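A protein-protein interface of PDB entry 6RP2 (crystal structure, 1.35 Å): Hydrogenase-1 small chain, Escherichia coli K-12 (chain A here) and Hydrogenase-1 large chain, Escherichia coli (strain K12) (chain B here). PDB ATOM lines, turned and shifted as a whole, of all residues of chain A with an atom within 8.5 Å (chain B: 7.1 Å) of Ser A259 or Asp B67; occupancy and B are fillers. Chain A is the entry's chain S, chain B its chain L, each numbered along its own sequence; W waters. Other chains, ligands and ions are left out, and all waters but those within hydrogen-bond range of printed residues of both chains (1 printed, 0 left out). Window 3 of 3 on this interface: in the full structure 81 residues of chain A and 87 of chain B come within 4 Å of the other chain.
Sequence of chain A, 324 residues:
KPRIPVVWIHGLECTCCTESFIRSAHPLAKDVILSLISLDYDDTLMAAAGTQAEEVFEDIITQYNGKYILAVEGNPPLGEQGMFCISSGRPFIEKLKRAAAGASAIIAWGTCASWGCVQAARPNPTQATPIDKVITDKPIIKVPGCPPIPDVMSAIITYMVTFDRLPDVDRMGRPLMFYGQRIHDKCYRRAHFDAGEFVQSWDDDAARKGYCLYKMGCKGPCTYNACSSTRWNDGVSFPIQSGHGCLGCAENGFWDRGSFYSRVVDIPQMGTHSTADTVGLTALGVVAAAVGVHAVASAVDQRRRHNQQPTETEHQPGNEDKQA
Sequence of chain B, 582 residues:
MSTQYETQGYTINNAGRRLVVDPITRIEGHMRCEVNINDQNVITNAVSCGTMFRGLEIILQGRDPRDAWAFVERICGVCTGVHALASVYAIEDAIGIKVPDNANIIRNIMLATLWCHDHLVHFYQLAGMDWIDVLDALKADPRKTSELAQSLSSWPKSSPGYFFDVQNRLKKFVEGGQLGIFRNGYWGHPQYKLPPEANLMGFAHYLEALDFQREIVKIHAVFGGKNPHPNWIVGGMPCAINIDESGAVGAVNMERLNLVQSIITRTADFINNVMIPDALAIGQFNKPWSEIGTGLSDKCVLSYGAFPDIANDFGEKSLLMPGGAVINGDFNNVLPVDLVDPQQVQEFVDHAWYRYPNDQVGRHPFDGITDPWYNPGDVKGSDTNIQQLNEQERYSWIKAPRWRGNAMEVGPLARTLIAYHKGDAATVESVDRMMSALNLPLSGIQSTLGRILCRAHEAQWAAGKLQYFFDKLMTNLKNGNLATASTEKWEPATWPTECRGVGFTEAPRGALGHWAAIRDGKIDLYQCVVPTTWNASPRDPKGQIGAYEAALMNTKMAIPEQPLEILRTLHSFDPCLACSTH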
ATOM      1  N   MET A 216      -9.866  -7.518   2.226  1.00  0.00           N
ATOM      2  CA  MET A 216     -10.953  -6.672   1.696  1.00  0.00           C
ATOM      3  C   MET A 216     -11.859  -6.201   2.842  1.00  0.00           C
ATOM      4  O   MET A 216     -12.898  -5.546   2.550  1.00  0.00           O
ATOM      5  CB  MET A 216     -11.769  -7.430   0.637  1.00  0.00           C
ATOM      6  CG  MET A 216     -10.952  -7.914  -0.545  1.00  0.00           C
ATOM      7  SD  MET A 216      -9.867  -6.656  -1.273  1.00  0.00           S
ATOM      8  CE  MET A 216     -11.057  -5.453  -1.876  1.00  0.00           C
ATOM      9  N   GLY A 217     -11.470  -6.430   4.102  1.00  0.00           N
ATOM     10  CA  GLY A 217     -12.144  -5.871   5.283  1.00  0.00           C
ATOM     11  C   GLY A 217     -13.108  -6.818   5.986  1.00  0.00           C
ATOM     12  O   GLY A 217     -13.826  -6.385   6.895  1.00  0.00           O
ATOM     13  N   CYS A 218     -13.087  -8.093   5.648  1.00  0.00           N
ATOM     14  CA  CYS A 218     -14.058  -9.037   6.260  1.00  0.00           C
ATOM     15  C   CYS A 218     -13.982  -8.961   7.789  1.00  0.00           C
ATOM     16  O   CYS A 218     -12.909  -9.127   8.392  1.00  0.00           O
ATOM     17  CB  CYS A 218     -13.729 -10.462   5.832  1.00  0.00           C
ATOM     18  SG  CYS A 218     -14.931 -11.666   6.434  1.00  0.00           S
ATOM     19  N   LYS A 219     -15.137  -8.801   8.407  1.00  0.00           N
ATOM     20  CA  LYS A 219     -15.256  -8.732   9.879  1.00  0.00           C
ATOM     21  C   LYS A 219     -15.678 -10.055  10.488  1.00  0.00           C
ATOM     22  O   LYS A 219     -15.961 -10.128  11.696  1.00  0.00           O
ATOM     23  CB  LYS A 219     -16.177  -7.572  10.258  1.00  0.00           C
ATOM     24  CG  LYS A 219     -15.629  -6.196   9.824  1.00  0.00           C
ATOM     25  CD  LYS A 219     -14.131  -6.013  10.113  1.00  0.00           C
ATOM     26  CE  LYS A 219     -13.505  -4.660   9.868  1.00  0.00           C
ATOM     27  NZ  LYS A 219     -13.823  -4.080   8.561  1.00  0.00           N
ATOM     28  N   HIS A 244     -18.442 -10.711  -0.819  1.00  0.00           N
ATOM     29  CA  HIS A 244     -18.227  -9.518   0.034  1.00  0.00           C
ATOM     30  C   HIS A 244     -17.831  -9.977   1.424  1.00  0.00           C
ATOM     31  O   HIS A 244     -18.445 -10.892   1.997  1.00  0.00           O
ATOM     32  CB  HIS A 244     -19.461  -8.625   0.098  1.00  0.00           C
ATOM     33  CG  HIS A 244     -19.173  -7.226   0.517  1.00  0.00           C
ATOM     34  ND1 HIS A 244     -18.846  -6.861   1.811  1.00  0.00           N
ATOM     35  CD2 HIS A 244     -19.167  -6.105  -0.200  1.00  0.00           C
ATOM     36  CE1 HIS A 244     -18.615  -5.553   1.824  1.00  0.00           C
ATOM     37  NE2 HIS A 244     -18.787  -5.046   0.594  1.00  0.00           N
ATOM     38  N   CYS A 246     -17.849 -10.082   5.424  1.00  0.00           N
ATOM     39  CA  CYS A 246     -18.778  -9.773   6.546  1.00  0.00           C
ATOM     40  C   CYS A 246     -18.581  -8.318   6.963  1.00  0.00           C
ATOM     41  O   CYS A 246     -17.429  -7.849   7.069  1.00  0.00           O
ATOM     42  CB  CYS A 246     -18.516 -10.762   7.671  1.00  0.00           C
ATOM     43  SG  CYS A 246     -19.454 -10.521   9.207  1.00  0.00           S
ATOM     44  N   LEU A 247     -19.676  -7.582   7.090  1.00  0.00           N
ATOM     45  CA  LEU A 247     -19.698  -6.214   7.618  1.00  0.00           C
ATOM     46  C   LEU A 247     -19.615  -6.222   9.124  1.00  0.00           C
ATOM     47  O   LEU A 247     -19.368  -5.111   9.692  1.00  0.00           O
ATOM     48  CB  LEU A 247     -20.992  -5.534   7.206  1.00  0.00           C
ATOM     49  CG  LEU A 247     -21.364  -5.547   5.732  1.00  0.00           C
ATOM     50  CD1 LEU A 247     -22.690  -4.866   5.533  1.00  0.00           C
ATOM     51  CD2 LEU A 247     -20.323  -4.834   4.869  1.00  0.00           C
ATOM     52  N   PHE A 254     -21.270  -2.070  15.116  1.00  0.00           N
ATOM     53  CA  PHE A 254     -20.486  -2.495  13.949  1.00  0.00           C
ATOM     54  C   PHE A 254     -20.360  -1.382  12.928  1.00  0.00           C
ATOM     55  O   PHE A 254     -19.333  -1.355  12.195  1.00  0.00           O
ATOM     56  CB  PHE A 254     -21.030  -3.756  13.289  1.00  0.00           C
ATOM     57  CG  PHE A 254     -22.243  -3.606  12.422  1.00  0.00           C
ATOM     58  CD1 PHE A 254     -23.535  -3.566  12.950  1.00  0.00           C
ATOM     59  CD2 PHE A 254     -22.134  -3.468  11.042  1.00  0.00           C
ATOM     60  CE1 PHE A 254     -24.646  -3.462  12.115  1.00  0.00           C
ATOM     61  CE2 PHE A 254     -23.250  -3.335  10.223  1.00  0.00           C
ATOM     62  CZ  PHE A 254     -24.500  -3.328  10.765  1.00  0.00           C
ATOM     63  N   TRP A 255     -21.293  -0.456  12.836  1.00  0.00           N
ATOM     64  CA  TRP A 255     -21.232   0.683  11.893  1.00  0.00           C
ATOM     65  C   TRP A 255     -20.039   1.588  12.180  1.00  0.00           C
ATOM     66  O   TRP A 255     -19.591   2.246  11.237  1.00  0.00           O
ATOM     67  CB  TRP A 255     -22.517   1.482  11.943  1.00  0.00           C
ATOM     68  CG  TRP A 255     -23.747   0.716  11.569  1.00  0.00           C
ATOM     69  CD1 TRP A 255     -24.687   0.170  12.414  1.00  0.00           C
ATOM     70  CD2 TRP A 255     -24.177   0.360  10.241  1.00  0.00           C
ATOM     71  NE1 TRP A 255     -25.667  -0.426  11.688  1.00  0.00           N
ATOM     72  CE2 TRP A 255     -25.377  -0.357  10.359  1.00  0.00           C
ATOM     73  CE3 TRP A 255     -23.682   0.587   8.963  1.00  0.00           C
ATOM     74  CZ2 TRP A 255     -26.066  -0.856   9.251  1.00  0.00           C
ATOM     75  CZ3 TRP A 255     -24.354   0.068   7.874  1.00  0.00           C
ATOM     76  CH2 TRP A 255     -25.534  -0.635   8.019  1.00  0.00           C
ATOM     77  N   ASP A 256     -19.582   1.618  13.415  1.00  0.00           N
ATOM     78  CA  ASP A 256     -18.568   2.589  13.866  1.00  0.00           C
ATOM     79  C   ASP A 256     -17.238   1.930  14.190  1.00  0.00           C
ATOM     80  O   ASP A 256     -16.377   2.574  14.793  1.00  0.00           O
ATOM     81  CB  ASP A 256     -19.141   3.407  15.013  1.00  0.00           C
ATOM     82  CG  ASP A 256     -20.197   4.401  14.591  1.00  0.00           C
ATOM     83  OD1 ASP A 256     -20.097   4.989  13.500  1.00  0.00           O
ATOM     84  OD2 ASP A 256     -21.115   4.624  15.370  1.00  0.00           O
ATOM     85  N   ARG A 257     -17.044   0.712  13.724  1.00  0.00           N
ATOM     86  CA  ARG A 257     -15.724   0.042  13.884  1.00  0.00           C
ATOM     87  C   ARG A 257     -14.838   0.289  12.664  1.00  0.00           C
ATOM     88  O   ARG A 257     -13.997  -0.620  12.314  1.00  0.00           O
ATOM     89  CB  ARG A 257     -15.957  -1.456  14.005  1.00  0.00           C
ATOM     90  CG  ARG A 257     -16.738  -1.841  15.239  1.00  0.00           C
ATOM     91  CD  ARG A 257     -15.888  -2.172  16.455  1.00  0.00           C
ATOM     92  NE  ARG A 257     -16.834  -2.430  17.544  1.00  0.00           N
ATOM     93  CZ  ARG A 257     -17.065  -1.640  18.602  1.00  0.00           C
ATOM     94  NH1 ARG A 257     -16.395  -0.512  18.787  1.00  0.00           N
ATOM     95  NH2 ARG A 257     -17.977  -1.998  19.496  1.00  0.00           N
ATOM     96  N   GLY A 258     -14.937   1.412  12.006  1.00  0.00           N
ATOM     97  CA  GLY A 258     -14.099   1.707  10.860  1.00  0.00           C
ATOM     98  C   GLY A 258     -14.756   1.254   9.572  1.00  0.00           C
ATOM     99  O   GLY A 258     -15.816   0.543   9.596  1.00  0.00           O
ATOM    100  N   SER A 259     -14.108   1.621   8.490  1.00  0.00           N
ATOM    101  CA  SER A 259     -14.556   1.281   7.120  1.00  0.00           C
ATOM    102  C   SER A 259     -14.760  -0.222   7.027  1.00  0.00           C
ATOM    103  O   SER A 259     -13.966  -1.001   7.536  1.00  0.00           O
ATOM    104  CB  SER A 259     -13.608   1.753   6.077  1.00  0.00           C
ATOM    105  OG  SER A 259     -13.989   1.310   4.768  1.00  0.00           O
ATOM    106  N   PHE A 260     -15.810  -0.629   6.336  1.00  0.00           N
ATOM    107  CA  PHE A 260     -16.048  -2.064   6.085  1.00  0.00           C
ATOM    108  C   PHE A 260     -14.874  -2.627   5.292  1.00  0.00           C
ATOM    109  O   PHE A 260     -14.713  -3.849   5.282  1.00  0.00           O
ATOM    110  CB  PHE A 260     -17.376  -2.256   5.352  1.00  0.00           C
ATOM    111  CG  PHE A 260     -18.562  -1.865   6.208  1.00  0.00           C
ATOM    112  CD1 PHE A 260     -18.704  -2.392   7.474  1.00  0.00           C
ATOM    113  CD2 PHE A 260     -19.473  -0.942   5.739  1.00  0.00           C
ATOM    114  CE1 PHE A 260     -19.788  -2.042   8.265  1.00  0.00           C
ATOM    115  CE2 PHE A 260     -20.545  -0.593   6.539  1.00  0.00           C
ATOM    116  CZ  PHE A 260     -20.677  -1.117   7.791  1.00  0.00           C
ATOM    117  N   TYR A 261     -14.109  -1.790   4.590  1.00  0.00           N
ATOM    118  CA  TYR A 261     -12.996  -2.249   3.734  1.00  0.00           C
ATOM    119  C   TYR A 261     -11.646  -2.143   4.452  1.00  0.00           C
ATOM    120  O   TYR A 261     -10.643  -2.507   3.829  1.00  0.00           O
ATOM    121  CB  TYR A 261     -13.053  -1.566   2.371  1.00  0.00           C
ATOM    122  CG  TYR A 261     -14.401  -1.776   1.757  1.00  0.00           C
ATOM    123  CD1 TYR A 261     -14.767  -3.035   1.326  1.00  0.00           C
ATOM    124  CD2 TYR A 261     -15.330  -0.746   1.651  1.00  0.00           C
ATOM    125  CE1 TYR A 261     -16.037  -3.268   0.835  1.00  0.00           C
ATOM    126  CE2 TYR A 261     -16.605  -0.962   1.145  1.00  0.00           C
ATOM    127  CZ  TYR A 261     -16.915  -2.213   0.663  1.00  0.00           C
ATOM    128  OH  TYR A 261     -18.173  -2.429   0.158  1.00  0.00           O
ATOM    129  N   SER A 262     -11.608  -1.739   5.712  1.00  0.00           N
ATOM    130  CA  SER A 262     -10.355  -1.770   6.521  1.00  0.00           C
ATOM    131  C   SER A 262     -10.249  -3.113   7.237  1.00  0.00           C
ATOM    132  O   SER A 262     -11.211  -3.583   7.823  1.00  0.00           O
ATOM    133  CB  SER A 262     -10.255  -0.648   7.472  1.00  0.00           C
ATOM    134  OG  SER A 262     -10.245   0.565   6.756  1.00  0.00           O
ATOM    135  N   ARG A 263      -9.081  -3.728   7.203  1.00  0.00           N
ATOM    136  CA  ARG A 263      -8.910  -5.069   7.790  1.00  0.00           C
ATOM    137  C   ARG A 263      -9.017  -4.978   9.309  1.00  0.00           C
ATOM    138  O   ARG A 263      -8.734  -3.916   9.922  1.00  0.00           O
ATOM    139  CB  ARG A 263      -7.648  -5.758   7.276  1.00  0.00           C
ATOM    140  CG  ARG A 263      -6.358  -5.123   7.739  1.00  0.00           C
ATOM    141  CD  ARG A 263      -5.278  -5.913   6.989  1.00  0.00           C
ATOM    142  NE  ARG A 263      -5.194  -5.518   5.583  1.00  0.00           N
ATOM    143  CZ  ARG A 263      -4.168  -5.832   4.772  1.00  0.00           C
ATOM    144  NH1 ARG A 263      -3.194  -6.601   5.221  1.00  0.00           N
ATOM    145  NH2 ARG A 263      -4.138  -5.412   3.527  1.00  0.00           N
ATOM    146  N   VAL A 264      -9.470  -6.065   9.914  1.00  0.00           N
ATOM    147  CA  VAL A 264      -9.526  -6.198  11.408  1.00  0.00           C
ATOM    148  C   VAL A 264      -8.155  -5.872  12.018  1.00  0.00           C
ATOM    149  O   VAL A 264      -7.328  -6.568  11.447  1.00  0.00           O
ATOM    150  CB  VAL A 264      -9.967  -7.621  11.804  1.00  0.00           C
ATOM    151  CG1 VAL A 264      -9.720  -7.932  13.289  1.00  0.00           C
ATOM    152  CG2 VAL A 264     -11.407  -7.875  11.459  1.00  0.00           C
ATOM    153  N   LEU B  60     -24.330   9.730   7.534  1.00  0.00           N
ATOM    154  CA  LEU B  60     -23.455   9.493   6.368  1.00  0.00           C
ATOM    155  C   LEU B  60     -22.300  10.492   6.324  1.00  0.00           C
ATOM    156  O   LEU B  60     -21.292  10.238   5.642  1.00  0.00           O
ATOM    157  CB  LEU B  60     -24.265   9.548   5.084  1.00  0.00           C
ATOM    158  CG  LEU B  60     -24.714   8.196   4.543  1.00  0.00           C
ATOM    159  CD1 LEU B  60     -23.554   7.400   4.007  1.00  0.00           C
ATOM    160  CD2 LEU B  60     -25.415   7.313   5.561  1.00  0.00           C
ATOM    161  N   ARG B  63     -18.355   9.523   6.421  1.00  0.00           N
ATOM    162  CA  ARG B  63     -18.104   8.119   6.061  1.00  0.00           C
ATOM    163  C   ARG B  63     -17.229   8.074   4.810  1.00  0.00           C
ATOM    164  O   ARG B  63     -17.236   8.983   3.969  1.00  0.00           O
ATOM    165  CB  ARG B  63     -19.426   7.401   5.812  1.00  0.00           C
ATOM    166  CG  ARG B  63     -20.375   7.401   6.994  1.00  0.00           C
ATOM    167  CD  ARG B  63     -19.822   6.764   8.234  1.00  0.00           C
ATOM    168  NE  ARG B  63     -20.711   6.968   9.389  1.00  0.00           N
ATOM    169  CZ  ARG B  63     -20.560   6.357  10.535  1.00  0.00           C
ATOM    170  NH1 ARG B  63     -19.632   5.421  10.671  1.00  0.00           N
ATOM    171  NH2 ARG B  63     -21.362   6.622  11.557  1.00  0.00           N
ATOM    172  N   ASP B  64     -16.578   6.938   4.613  1.00  0.00           N
ATOM    173  CA  ASP B  64     -15.902   6.657   3.333  1.00  0.00           C
ATOM    174  C   ASP B  64     -16.953   6.453   2.254  1.00  0.00           C
ATOM    175  O   ASP B  64     -17.931   5.701   2.452  1.00  0.00           O
ATOM    176  CB  ASP B  64     -15.004   5.432   3.484  1.00  0.00           C
ATOM    177  CG  ASP B  64     -14.064   5.178   2.300  1.00  0.00           C
ATOM    178  OD1 ASP B  64     -14.569   5.028   1.173  1.00  0.00           O
ATOM    179  OD2 ASP B  64     -12.838   5.219   2.518  1.00  0.00           O
ATOM    180  N   PRO B  65     -16.870   7.111   1.086  1.00  0.00           N
ATOM    181  CA  PRO B  65     -17.870   6.924   0.033  1.00  0.00           C
ATOM    182  C   PRO B  65     -18.083   5.448  -0.340  1.00  0.00           C
ATOM    183  O   PRO B  65     -19.186   5.093  -0.756  1.00  0.00           O
ATOM    184  CB  PRO B  65     -17.264   7.720  -1.144  1.00  0.00           C
ATOM    185  CG  PRO B  65     -16.497   8.812  -0.426  1.00  0.00           C
ATOM    186  CD  PRO B  65     -15.854   8.114   0.739  1.00  0.00           C
ATOM    187  N   ARG B  66     -17.065   4.612  -0.228  1.00  0.00           N
ATOM    188  CA  ARG B  66     -17.185   3.170  -0.583  1.00  0.00           C
ATOM    189  C   ARG B  66     -18.113   2.455   0.386  1.00  0.00           C
ATOM    190  O   ARG B  66     -18.659   1.414   0.015  1.00  0.00           O
ATOM    191  CB  ARG B  66     -15.816   2.511  -0.641  1.00  0.00           C
ATOM    192  CG  ARG B  66     -14.935   3.085  -1.753  1.00  0.00           C
ATOM    193  CD  ARG B  66     -13.476   2.693  -1.666  1.00  0.00           C
ATOM    194  NE  ARG B  66     -12.835   3.242  -0.501  1.00  0.00           N
ATOM    195  CZ  ARG B  66     -11.636   2.888  -0.067  1.00  0.00           C
ATOM    196  NH1 ARG B  66     -10.917   2.011  -0.747  1.00  0.00           N
ATOM    197  NH2 ARG B  66     -11.196   3.356   1.072  1.00  0.00           N
ATOM    198  N   ASP B  67     -18.244   2.951   1.610  1.00  0.00           N
ATOM    199  CA  ASP B  67     -19.096   2.333   2.653  1.00  0.00           C
ATOM    200  C   ASP B  67     -20.534   2.824   2.550  1.00  0.00           C
ATOM    201  O   ASP B  67     -21.408   2.203   3.197  1.00  0.00           O
ATOM    202  CB  ASP B  67     -18.545   2.649   4.035  1.00  0.00           C
ATOM    203  CG  ASP B  67     -17.208   2.010   4.316  1.00  0.00           C
ATOM    204  OD1 ASP B  67     -17.179   0.730   4.243  1.00  0.00           O
ATOM    205  OD2 ASP B  67     -16.219   2.761   4.686  1.00  0.00           O
ATOM    206  N   ALA B  68     -20.783   3.920   1.823  1.00  0.00           N
ATOM    207  CA  ALA B  68     -22.072   4.610   1.939  1.00  0.00           C
ATOM    208  C   ALA B  68     -23.252   3.674   1.630  1.00  0.00           C
ATOM    209  O   ALA B  68     -24.329   3.750   2.290  1.00  0.00           O
ATOM    210  CB  ALA B  68     -22.088   5.819   1.070  1.00  0.00           C
ATOM    211  N   TRP B  69     -23.096   2.822   0.614  1.00  0.00           N
ATOM    212  CA  TRP B  69     -24.214   1.975   0.142  1.00  0.00           C
ATOM    213  C   TRP B  69     -24.767   1.150   1.310  1.00  0.00           C
ATOM    214  O   TRP B  69     -25.981   0.897   1.351  1.00  0.00           O
ATOM    215  CB  TRP B  69     -23.771   1.100  -1.032  1.00  0.00           C
ATOM    216  CG  TRP B  69     -22.774   0.050  -0.659  1.00  0.00           C
ATOM    217  CD1 TRP B  69     -21.424   0.165  -0.736  1.00  0.00           C
ATOM    218  CD2 TRP B  69     -23.045  -1.216  -0.046  1.00  0.00           C
ATOM    219  NE1 TRP B  69     -20.830  -0.952  -0.226  1.00  0.00           N
ATOM    220  CE2 TRP B  69     -21.793  -1.802   0.226  1.00  0.00           C
ATOM    221  CE3 TRP B  69     -24.210  -1.895   0.308  1.00  0.00           C
ATOM    222  CZ2 TRP B  69     -21.668  -3.043   0.838  1.00  0.00           C
ATOM    223  CZ3 TRP B  69     -24.074  -3.107   0.946  1.00  0.00           C
ATOM    224  CH2 TRP B  69     -22.840  -3.660   1.222  1.00  0.00           C
ATOM    225  N   ALA B  70     -23.874   0.669   2.183  1.00  0.00           N
ATOM    226  CA  ALA B  70     -24.257  -0.287   3.235  1.00  0.00           C
ATOM    227  C   ALA B  70     -25.120   0.428   4.271  1.00  0.00           C
ATOM    228  O   ALA B  70     -26.070  -0.164   4.777  1.00  0.00           O
ATOM    229  CB  ALA B  70     -23.037  -0.906   3.830  1.00  0.00           C
ATOM    230  N   PHE B  71     -24.771   1.684   4.584  1.00  0.00           N
ATOM    231  CA  PHE B  71     -25.543   2.530   5.511  1.00  0.00           C
ATOM    232  C   PHE B  71     -26.916   2.845   4.936  1.00  0.00           C
ATOM    233  O   PHE B  71     -27.954   2.612   5.549  1.00  0.00           O
ATOM    234  CB  PHE B  71     -24.764   3.803   5.820  1.00  0.00           C
ATOM    235  CG  PHE B  71     -23.630   3.640   6.797  1.00  0.00           C
ATOM    236  CD1 PHE B  71     -22.376   3.206   6.383  1.00  0.00           C
ATOM    237  CD2 PHE B  71     -23.749   4.128   8.102  1.00  0.00           C
ATOM    238  CE1 PHE B  71     -21.333   3.077   7.289  1.00  0.00           C
ATOM    239  CE2 PHE B  71     -22.701   4.020   8.993  1.00  0.00           C
ATOM    240  CZ  PHE B  71     -21.502   3.476   8.582  1.00  0.00           C
ATOM    241  N   VAL B  72     -26.935   3.385   3.722  1.00  0.00           N
ATOM    242  CA  VAL B  72     -28.196   3.888   3.137  1.00  0.00           C
ATOM    243  C   VAL B  72     -29.058   2.718   2.693  1.00  0.00           C
ATOM    244  O   VAL B  72     -30.279   2.891   2.627  1.00  0.00           O
ATOM    245  CB  VAL B  72     -28.005   4.943   2.042  1.00  0.00           C
ATOM    246  CG1 VAL B  72     -27.389   6.200   2.614  1.00  0.00           C
ATOM    247  CG2 VAL B  72     -27.226   4.429   0.848  1.00  0.00           C
ATOM    248  N   SER B  87     -26.870   4.590  -4.270  1.00  0.00           N
ATOM    249  CA  SER B  87     -25.623   5.038  -3.627  1.00  0.00           C
ATOM    250  C   SER B  87     -24.433   4.733  -4.510  1.00  0.00           C
ATOM    251  O   SER B  87     -23.588   5.615  -4.736  1.00  0.00           O
ATOM    252  CB  SER B  87     -25.463   4.411  -2.264  1.00  0.00           C
ATOM    253  OG  SER B  87     -24.320   4.916  -1.573  1.00  0.00           O
ATOM    254  N   ILE B  91     -21.895   7.608  -6.040  1.00  0.00           N
ATOM    255  CA  ILE B  91     -20.450   7.693  -5.768  1.00  0.00           C
ATOM    256  C   ILE B  91     -19.712   7.515  -7.095  1.00  0.00           C
ATOM    257  O   ILE B  91     -18.688   8.183  -7.303  1.00  0.00           O
ATOM    258  CB  ILE B  91     -20.077   6.659  -4.705  1.00  0.00           C
ATOM    259  CG1 ILE B  91     -20.846   6.944  -3.402  1.00  0.00           C
ATOM    260  CG2 ILE B  91     -18.569   6.626  -4.501  1.00  0.00           C
ATOM    261  CD1 ILE B  91     -20.793   8.365  -2.912  1.00  0.00           C
ATOM    262  N   VAL B 234     -18.925  -0.156  -4.826  1.00  0.00           N
ATOM    263  CA  VAL B 234     -18.520   0.915  -5.757  1.00  0.00           C
ATOM    264  C   VAL B 234     -17.540   0.296  -6.750  1.00  0.00           C
ATOM    265  O   VAL B 234     -16.543  -0.306  -6.309  1.00  0.00           O
ATOM    266  CB  VAL B 234     -17.917   2.093  -4.997  1.00  0.00           C
ATOM    267  CG1 VAL B 234     -17.325   3.092  -5.966  1.00  0.00           C
ATOM    268  CG2 VAL B 234     -18.956   2.746  -4.089  1.00  0.00           C
ATOM    269  N   TRP B 490     -10.650   2.540  -7.147  1.00  0.00           N
ATOM    270  CA  TRP B 490     -11.031   2.047  -5.801  1.00  0.00           C
ATOM    271  C   TRP B 490     -10.303   2.851  -4.720  1.00  0.00           C
ATOM    272  O   TRP B 490     -10.895   3.173  -3.698  1.00  0.00           O
ATOM    273  CB  TRP B 490     -10.763   0.538  -5.703  1.00  0.00           C
ATOM    274  CG  TRP B 490     -11.014  -0.044  -4.353  1.00  0.00           C
ATOM    275  CD1 TRP B 490     -10.071  -0.431  -3.473  1.00  0.00           C
ATOM    276  CD2 TRP B 490     -12.298  -0.272  -3.719  1.00  0.00           C
ATOM    277  NE1 TRP B 490     -10.660  -0.908  -2.332  1.00  0.00           N
ATOM    278  CE2 TRP B 490     -12.014  -0.797  -2.445  1.00  0.00           C
ATOM    279  CE3 TRP B 490     -13.640  -0.031  -4.054  1.00  0.00           C
ATOM    280  CZ2 TRP B 490     -13.031  -1.135  -1.549  1.00  0.00           C
ATOM    281  CZ3 TRP B 490     -14.653  -0.375  -3.189  1.00  0.00           C
ATOM    282  CH2 TRP B 490     -14.335  -0.926  -1.940  1.00  0.00           C
ATOM    283  N   LYS B 522     -13.862  11.765   1.971  1.00  0.00           N
ATOM    284  CA  LYS B 522     -15.016  11.477   2.865  1.00  0.00           C
ATOM    285  C   LYS B 522     -16.266  12.160   2.356  1.00  0.00           C
ATOM    286  O   LYS B 522     -16.214  13.120   1.595  1.00  0.00           O
ATOM    287  CB  LYS B 522     -14.712  11.991   4.265  1.00  0.00           C
ATOM    288  CG  LYS B 522     -13.491  11.385   4.926  1.00  0.00           C
ATOM    289  CD  LYS B 522     -13.602   9.906   5.160  1.00  0.00           C
ATOM    290  CE  LYS B 522     -12.534   9.458   6.126  1.00  0.00           C
ATOM    291  NZ  LYS B 522     -11.715   8.425   5.521  1.00  0.00           N
HETATM  292  O   HOH W   1     -17.932  -0.336  -1.983  1.00  0.00           O
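O of Trp A255 is in hydrogen-bond range of NH1 of Arg B63, 3.2 Å away.
The guanidinium group of Arg B63 is in salt-bridge range of the side-chain carboxylate of Asp A256.
OG of Ser A259 lies within hydrogen-bond range of OD2 of Asp B67, 2.7 Å away.
OD1 of Asp B67 lies within hydrogen-bond range of N of Phe A260, at 2.8 Å.
OH of Tyr A261 lies within hydrogen-bond range of NE1 of Trp B69, 3.1 Å away.
NZ of Lys A219 lies within hydrogen-bond range of O of Ser A259 (3.2 Å).
The side-chain amino group (NZ) of Lys A219 is in hydrogen-bond range of the backbone carbonyl oxygen (O) of Phe A260, at 3.4 Å.
NH2 of Arg B66 is in salt-bridge range of OD2 of Asp B64.
O of Arg B66 sits close to NE1 of Trp B69, 3.2 Å away.
The guanidinium group (NH1) of Arg B66 sits at hydrogen-bond distance from the backbone carbonyl oxygen (O) of Trp B490.
N of Trp B69 sits at hydrogen-bond distance from OG of Ser B87 (3.3 Å).
Among the printed residues, pairs that only touch across the chains: His A244 with Trp B69 (3.5 Å), Trp A255 with Ala B70 (3.3 Å), Trp A255 with Phe B71 (3.5 Å), Phe A260 with Ala B70 (3.7 Å), Phe A260 with Phe B71 (3.8 Å), Tyr A261 with Arg B66 (3.3 Å), Tyr A261 with Asp B67 (3.5 Å) and Tyr A261 with Trp B490 (3.6 Å).
Of the printed residues of chain B, Asp A256 touches Arg B63.
Printed residues of chain B within 4 Å of Ser A259: Asp B67 (2.7 Å).
Ser A262 touches none of the printed residues of chain B.
Of the printed residues of chain A, Arg B66 touches Tyr A261.
Of the printed residues of chain A, Asp B67 touches Ser A259 (2.7 Å), Phe A260 (2.8 Å) and Tyr A261 (3.5 Å).
No residue of chain A comes within 4 Å of Ala B68.
Of the printed residues of chain A, Trp B69 touches His A244 and Tyr A261.
The nearest printed residue of chain B that does not touch Ser A259 is Asp B64 (4.4 Å).
The nearest printed residue of chain A that does not touch Asp B67 is Gly A258 (5.3 Å).
Hydrophobic or aromatic side chains of chain B that line the printed part of chain A: Trp B69, Ala B70, Phe B71 and Trp B490.
Printed residues of chain A that touch a printed residue of chain B: His A244, Trp A255, Asp A256, Ser A259, Phe A260 and Tyr A261.
Among the printed residues, 13 pairs touch across the chains.
Among the printed residues, Asp or Glu carboxylates within 4 Å of a Lys or Arg side-chain nitrogen of the other chain: Asp A256 with Arg B63.
Water W1 lies within hydrogen-bond range of O of Arg B66 (2.8 Å), OH of Tyr A261 (3.0 Å), N of Val B234 (3.0 Å) and NE1 of Trp B69 (3.4 Å).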
